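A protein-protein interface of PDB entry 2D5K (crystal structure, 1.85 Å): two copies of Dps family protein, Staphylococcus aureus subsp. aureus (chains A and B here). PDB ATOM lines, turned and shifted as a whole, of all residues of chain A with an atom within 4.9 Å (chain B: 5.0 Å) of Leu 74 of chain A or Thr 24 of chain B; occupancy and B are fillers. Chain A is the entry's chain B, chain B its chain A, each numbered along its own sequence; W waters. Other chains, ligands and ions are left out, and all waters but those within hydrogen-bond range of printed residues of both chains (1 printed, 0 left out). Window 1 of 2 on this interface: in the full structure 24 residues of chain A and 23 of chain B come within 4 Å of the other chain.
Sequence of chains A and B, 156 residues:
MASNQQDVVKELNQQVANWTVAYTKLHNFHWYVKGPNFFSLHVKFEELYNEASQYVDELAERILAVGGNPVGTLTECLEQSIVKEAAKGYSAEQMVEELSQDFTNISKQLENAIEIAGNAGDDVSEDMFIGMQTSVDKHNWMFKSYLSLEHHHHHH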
ATOM      1  N   THR A  20     -17.002  18.091 -20.898  1.00  0.00           N
ATOM      2  CA  THR A  20     -17.885  17.322 -21.760  1.00  0.00           C
ATOM      3  C   THR A  20     -18.814  18.349 -22.412  1.00  0.00           C
ATOM      4  O   THR A  20     -19.083  18.285 -23.608  1.00  0.00           O
ATOM      5  CB  THR A  20     -18.703  16.293 -20.962  1.00  0.00           C
ATOM      6  OG1 THR A  20     -17.818  15.294 -20.432  1.00  0.00           O
ATOM      7  CG2 THR A  20     -19.730  15.615 -21.859  1.00  0.00           C
ATOM      8  N   GLY A  72     -20.897   9.430 -16.256  1.00  0.00           N
ATOM      9  CA  GLY A  72     -20.996   8.828 -17.574  1.00  0.00           C
ATOM     10  C   GLY A  72     -22.186   9.151 -18.460  1.00  0.00           C
ATOM     11  O   GLY A  72     -22.486   8.381 -19.368  1.00  0.00           O
ATOM     12  N   THR A  73     -22.869  10.264 -18.213  1.00  0.00           N
ATOM     13  CA  THR A  73     -24.002  10.647 -19.048  1.00  0.00           C
ATOM     14  C   THR A  73     -23.973  12.147 -19.302  1.00  0.00           C
ATOM     15  O   THR A  73     -23.418  12.907 -18.509  1.00  0.00           O
ATOM     16  CB  THR A  73     -25.361  10.296 -18.397  1.00  0.00           C
ATOM     17  OG1 THR A  73     -25.599  11.159 -17.277  1.00  0.00           O
ATOM     18  CG2 THR A  73     -25.372   8.841 -17.944  1.00  0.00           C
ATOM     19  N   LEU A  74     -24.574  12.565 -20.410  1.00  0.00           N
ATOM     20  CA  LEU A  74     -24.624  13.977 -20.768  1.00  0.00           C
ATOM     21  C   LEU A  74     -25.558  14.732 -19.829  1.00  0.00           C
ATOM     22  O   LEU A  74     -25.321  15.895 -19.487  1.00  0.00           O
ATOM     23  CB  LEU A  74     -25.097  14.124 -22.215  1.00  0.00           C
ATOM     24  CG  LEU A  74     -24.175  13.453 -23.240  1.00  0.00           C
ATOM     25  CD1 LEU A  74     -24.819  13.485 -24.618  1.00  0.00           C
ATOM     26  CD2 LEU A  74     -22.829  14.169 -23.260  1.00  0.00           C
ATOM     27  N   THR A  75     -26.622  14.064 -19.406  1.00  0.00           N
ATOM     28  CA  THR A  75     -27.584  14.676 -18.502  1.00  0.00           C
ATOM     29  C   THR A  75     -26.891  15.095 -17.207  1.00  0.00           C
ATOM     30  O   THR A  75     -27.106  16.199 -16.706  1.00  0.00           O
ATOM     31  CB  THR A  75     -28.727  13.697 -18.167  1.00  0.00           C
ATOM     32  OG1 THR A  75     -29.324  13.230 -19.384  1.00  0.00           O
ATOM     33  CG2 THR A  75     -29.788  14.389 -17.318  1.00  0.00           C
ATOM     34  N   GLU A  76     -26.058  14.210 -16.666  1.00  0.00           N
ATOM     35  CA  GLU A  76     -25.338  14.505 -15.431  1.00  0.00           C
ATOM     36  C   GLU A  76     -24.329  15.632 -15.656  1.00  0.00           C
ATOM     37  O   GLU A  76     -24.181  16.521 -14.816  1.00  0.00           O
ATOM     38  CB  GLU A  76     -24.623  13.249 -14.918  1.00  0.00           C
ATOM     39  CG  GLU A  76     -25.568  12.178 -14.373  1.00  0.00           C
ATOM     40  CD  GLU A  76     -24.870  10.853 -14.111  1.00  0.00           C
ATOM     41  OE1 GLU A  76     -24.411  10.215 -15.083  1.00  0.00           O
ATOM     42  OE2 GLU A  76     -24.780  10.450 -12.931  1.00  0.00           O
ATOM     43  N   CYS A  77     -23.642  15.600 -16.794  1.00  0.00           N
ATOM     44  CA  CYS A  77     -22.664  16.634 -17.108  1.00  0.00           C
ATOM     45  C   CYS A  77     -23.315  18.018 -17.161  1.00  0.00           C
ATOM     46  O   CYS A  77     -22.785  18.984 -16.610  1.00  0.00           O
ATOM     47  CB  CYS A  77     -21.972  16.325 -18.437  1.00  0.00           C
ATOM     48  SG  CYS A  77     -20.801  14.933 -18.374  1.00  0.00           S
ATOM     49  N   LEU A  78     -24.468  18.114 -17.817  1.00  0.00           N
ATOM     50  CA  LEU A  78     -25.174  19.387 -17.922  1.00  0.00           C
ATOM     51  C   LEU A  78     -25.577  19.913 -16.548  1.00  0.00           C
ATOM     52  O   LEU A  78     -25.680  21.120 -16.342  1.00  0.00           O
ATOM     53  CB  LEU A  78     -26.423  19.235 -18.796  1.00  0.00           C
ATOM     54  CG  LEU A  78     -26.201  19.046 -20.299  1.00  0.00           C
ATOM     55  CD1 LEU A  78     -27.505  18.632 -20.975  1.00  0.00           C
ATOM     56  CD2 LEU A  78     -25.679  20.341 -20.901  1.00  0.00           C
ATOM     57  N   THR B  20     -23.542  11.846 -31.182  1.00  0.00           N
ATOM     58  CA  THR B  20     -23.057  12.701 -30.110  1.00  0.00           C
ATOM     59  C   THR B  20     -23.372  11.969 -28.797  1.00  0.00           C
ATOM     60  O   THR B  20     -22.562  11.954 -27.872  1.00  0.00           O
ATOM     61  CB  THR B  20     -23.753  14.077 -30.123  1.00  0.00           C
ATOM     62  OG1 THR B  20     -23.322  14.816 -31.273  1.00  0.00           O
ATOM     63  CG2 THR B  20     -23.411  14.867 -28.862  1.00  0.00           C
ATOM     64  N   VAL B  21     -24.546  11.347 -28.723  1.00  0.00           N
ATOM     65  CA  VAL B  21     -24.913  10.607 -27.517  1.00  0.00           C
ATOM     66  C   VAL B  21     -24.066   9.334 -27.435  1.00  0.00           C
ATOM     67  O   VAL B  21     -23.574   8.981 -26.365  1.00  0.00           O
ATOM     68  CB  VAL B  21     -26.417  10.227 -27.510  1.00  0.00           C
ATOM     69  CG1 VAL B  21     -26.732   9.349 -26.292  1.00  0.00           C
ATOM     70  CG2 VAL B  21     -27.273  11.493 -27.467  1.00  0.00           C
ATOM     71  N   ALA B  22     -23.878   8.664 -28.572  1.00  0.00           N
ATOM     72  CA  ALA B  22     -23.088   7.433 -28.625  1.00  0.00           C
ATOM     73  C   ALA B  22     -21.637   7.688 -28.235  1.00  0.00           C
ATOM     74  O   ALA B  22     -20.989   6.837 -27.628  1.00  0.00           O
ATOM     75  CB  ALA B  22     -23.148   6.829 -30.022  1.00  0.00           C
ATOM     76  N   TYR B  23     -21.137   8.864 -28.596  1.00  0.00           N
ATOM     77  CA  TYR B  23     -19.768   9.255 -28.278  1.00  0.00           C
ATOM     78  C   TYR B  23     -19.533   9.169 -26.769  1.00  0.00           C
ATOM     79  O   TYR B  23     -18.532   8.616 -26.312  1.00  0.00           O
ATOM     80  CB  TYR B  23     -19.521  10.686 -28.756  1.00  0.00           C
ATOM     81  CG  TYR B  23     -18.122  11.191 -28.489  1.00  0.00           C
ATOM     82  CD1 TYR B  23     -17.046  10.778 -29.275  1.00  0.00           C
ATOM     83  CD2 TYR B  23     -17.872  12.072 -27.439  1.00  0.00           C
ATOM     84  CE1 TYR B  23     -15.752  11.235 -29.022  1.00  0.00           C
ATOM     85  CE2 TYR B  23     -16.587  12.534 -27.177  1.00  0.00           C
ATOM     86  CZ  TYR B  23     -15.534  12.112 -27.970  1.00  0.00           C
ATOM     87  OH  TYR B  23     -14.265  12.572 -27.702  1.00  0.00           O
ATOM     88  N   THR B  24     -20.464   9.717 -25.994  1.00  0.00           N
ATOM     89  CA  THR B  24     -20.336   9.686 -24.543  1.00  0.00           C
ATOM     90  C   THR B  24     -20.651   8.301 -23.982  1.00  0.00           C
ATOM     91  O   THR B  24     -20.021   7.861 -23.019  1.00  0.00           O
ATOM     92  CB  THR B  24     -21.232  10.765 -23.890  1.00  0.00           C
ATOM     93  OG1 THR B  24     -20.650  12.054 -24.131  1.00  0.00           O
ATOM     94  CG2 THR B  24     -21.356  10.545 -22.383  1.00  0.00           C
ATOM     95  N   LYS B  25     -21.605   7.593 -24.579  1.00  0.00           N
ATOM     96  CA  LYS B  25     -21.901   6.259 -24.084  1.00  0.00           C
ATOM     97  C   LYS B  25     -20.692   5.351 -24.305  1.00  0.00           C
ATOM     98  O   LYS B  25     -20.395   4.494 -23.474  1.00  0.00           O
ATOM     99  CB  LYS B  25     -23.142   5.657 -24.763  1.00  0.00           C
ATOM    100  CG  LYS B  25     -23.446   4.243 -24.255  1.00  0.00           C
ATOM    101  CD  LYS B  25     -24.913   3.839 -24.425  1.00  0.00           C
ATOM    102  CE  LYS B  25     -25.304   3.612 -25.877  1.00  0.00           C
ATOM    103  NZ  LYS B  25     -26.734   3.170 -25.957  1.00  0.00           N
ATOM    104  N   LEU B  26     -19.993   5.539 -25.423  1.00  0.00           N
ATOM    105  CA  LEU B  26     -18.812   4.729 -25.707  1.00  0.00           C
ATOM    106  C   LEU B  26     -17.696   5.066 -24.717  1.00  0.00           C
ATOM    107  O   LEU B  26     -16.884   4.207 -24.373  1.00  0.00           O
ATOM    108  CB  LEU B  26     -18.353   4.946 -27.153  1.00  0.00           C
ATOM    109  CG  LEU B  26     -19.245   4.247 -28.187  1.00  0.00           C
ATOM    110  CD1 LEU B  26     -19.019   4.843 -29.567  1.00  0.00           C
ATOM    111  CD2 LEU B  26     -18.947   2.752 -28.188  1.00  0.00           C
ATOM    112  N   HIS B  27     -17.653   6.313 -24.257  1.00  0.00           N
ATOM    113  CA  HIS B  27     -16.648   6.692 -23.266  1.00  0.00           C
ATOM    114  C   HIS B  27     -17.008   5.969 -21.978  1.00  0.00           C
ATOM    115  O   HIS B  27     -16.147   5.415 -21.290  1.00  0.00           O
ATOM    116  CB  HIS B  27     -16.648   8.204 -23.012  1.00  0.00           C
ATOM    117  CG  HIS B  27     -15.690   8.955 -23.881  1.00  0.00           C
ATOM    118  ND1 HIS B  27     -15.972   9.287 -25.189  1.00  0.00           N
ATOM    119  CD2 HIS B  27     -14.431   9.393 -23.643  1.00  0.00           C
ATOM    120  CE1 HIS B  27     -14.927   9.897 -25.719  1.00  0.00           C
ATOM    121  NE2 HIS B  27     -13.978   9.973 -24.803  1.00  0.00           N
ATOM    122  N   ASN B  28     -18.299   5.981 -21.664  1.00  0.00           N
ATOM    123  CA  ASN B  28     -18.818   5.320 -20.477  1.00  0.00           C
ATOM    124  C   ASN B  28     -18.417   3.842 -20.491  1.00  0.00           C
ATOM    125  O   ASN B  28     -17.875   3.330 -19.512  1.00  0.00           O
ATOM    126  CB  ASN B  28     -20.346   5.463 -20.448  1.00  0.00           C
ATOM    127  CG  ASN B  28     -20.978   4.791 -19.244  1.00  0.00           C
ATOM    128  OD1 ASN B  28     -20.785   3.598 -19.014  1.00  0.00           O
ATOM    129  ND2 ASN B  28     -21.749   5.556 -18.474  1.00  0.00           N
ATOM    130  N   LEU B  74     -26.113  19.752 -26.391  1.00  0.00           N
ATOM    131  CA  LEU B  74     -26.403  18.414 -25.890  1.00  0.00           C
ATOM    132  C   LEU B  74     -27.899  18.234 -25.647  1.00  0.00           C
ATOM    133  O   LEU B  74     -28.450  17.152 -25.858  1.00  0.00           O
ATOM    134  CB  LEU B  74     -25.624  18.162 -24.597  1.00  0.00           C
ATOM    135  CG  LEU B  74     -24.104  18.107 -24.772  1.00  0.00           C
ATOM    136  CD1 LEU B  74     -23.429  18.025 -23.411  1.00  0.00           C
ATOM    137  CD2 LEU B  74     -23.732  16.897 -25.628  1.00  0.00           C
ATOM    138  N   LEU B  78     -29.970  15.116 -27.214  1.00  0.00           N
ATOM    139  CA  LEU B  78     -30.698  14.180 -26.370  1.00  0.00           C
ATOM    140  C   LEU B  78     -32.162  14.090 -26.797  1.00  0.00           C
ATOM    141  O   LEU B  78     -32.785  13.035 -26.686  1.00  0.00           O
ATOM    142  CB  LEU B  78     -30.605  14.606 -24.902  1.00  0.00           C
ATOM    143  CG  LEU B  78     -29.231  14.431 -24.246  1.00  0.00           C
ATOM    144  CD1 LEU B  78     -29.196  15.155 -22.908  1.00  0.00           C
ATOM    145  CD2 LEU B  78     -28.935  12.944 -24.065  1.00  0.00           C
ATOM    146  N   GLU B  85     -28.648   6.984 -23.353  1.00  0.00           N
ATOM    147  CA  GLU B  85     -27.424   7.171 -22.596  1.00  0.00           C
ATOM    148  C   GLU B  85     -27.237   5.891 -21.800  1.00  0.00           C
ATOM    149  O   GLU B  85     -28.202   5.164 -21.540  1.00  0.00           O
ATOM    150  CB  GLU B  85     -27.541   8.355 -21.638  1.00  0.00           C
ATOM    151  CG  GLU B  85     -27.823   9.679 -22.315  1.00  0.00           C
ATOM    152  CD  GLU B  85     -27.029  10.811 -21.704  1.00  0.00           C
ATOM    153  OE1 GLU B  85     -25.811  10.889 -21.974  1.00  0.00           O
ATOM    154  OE2 GLU B  85     -27.614  11.610 -20.948  1.00  0.00           O
HETATM  155  O   HOH W   1     -30.388  10.888 -20.448  1.00  0.00           O
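Printed residues of chain B within 4 Å of Gly 72 of chain A: Thr 24 (3.9 Å) and Asn 28 (3.1 Å). Of chain B, only Thr 24, Leu 74 and Glu 85 come within 4 Å of Leu 74 of chain A. Of the printed residues of chain B, Thr 75 of chain A touches Glu 85 (2.8 Å). Of the printed residues of chain A, Asn 28 of chain B touches Gly 72. Of the printed residues of chain A, Leu 74 of chain B touches Leu 74. The nearest residue of chain B that does not touch Leu 74 of chain A is Val 21 of chain B (4.1 Å).
Of the 12 printed residues of chain B, 4 touch a printed residue of chain A. Printed residues of chain B that touch a printed residue of chain A: Thr 24, Asn 28, Leu 74 and Glu 85. Hydrophobic or aromatic side chains of chain B that line the printed part of chain A: Leu 74. Among the printed residues, no Asp or Glu carboxylate lies within 4 Å of a Lys or Arg side-chain nitrogen of the other chain.
Water W1 bridges OG1 of Thr 75 of chain A and OE2 of Glu 85 of chain B.
Leu 74 of chain A touches its own counterpart, Leu 74 of chain B. 3 positions are printed for both chains.
The side-chain hydroxyl (OG1) of Thr 75 of chain A lies within hydrogen-bond range of the side-chain carboxylate (OE2) of Glu 85 of chain B (2.8 Å). ND2 of Asn 28 of chain B sits at hydrogen-bond distance from O of Gly 72 of chain A (3.1 Å). The backbone NH (N) of Leu 74 of chain A lies within hydrogen-bond range of the side-chain carboxylate (OE1) of Glu 85 of chain B (2.6 Å).
The side-chain sulfur of Cys 77 of chain A lies within hydrogen-bond range of the backbone carbonyl oxygen of Thr 73 of chain A (3.3 Å). The side-chain hydroxyl (OG1) of Thr 73 of chain A is in hydrogen-bond range of the side-chain carboxylate (OE1) of Glu 76 of chain A, at 2.7 Å.
Among the printed residues, merely in contact across the chains: Leu 74 of chain A with Thr 24 of chain B (3.2 Å), Thr 73 of chain A with Glu 85 of chain B (3.4 Å), Leu 74 of chain A with Leu 74 of chain B (3.7 Å) and Gly 72 of chain A with Thr 24 of chain B (3.9 Å).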
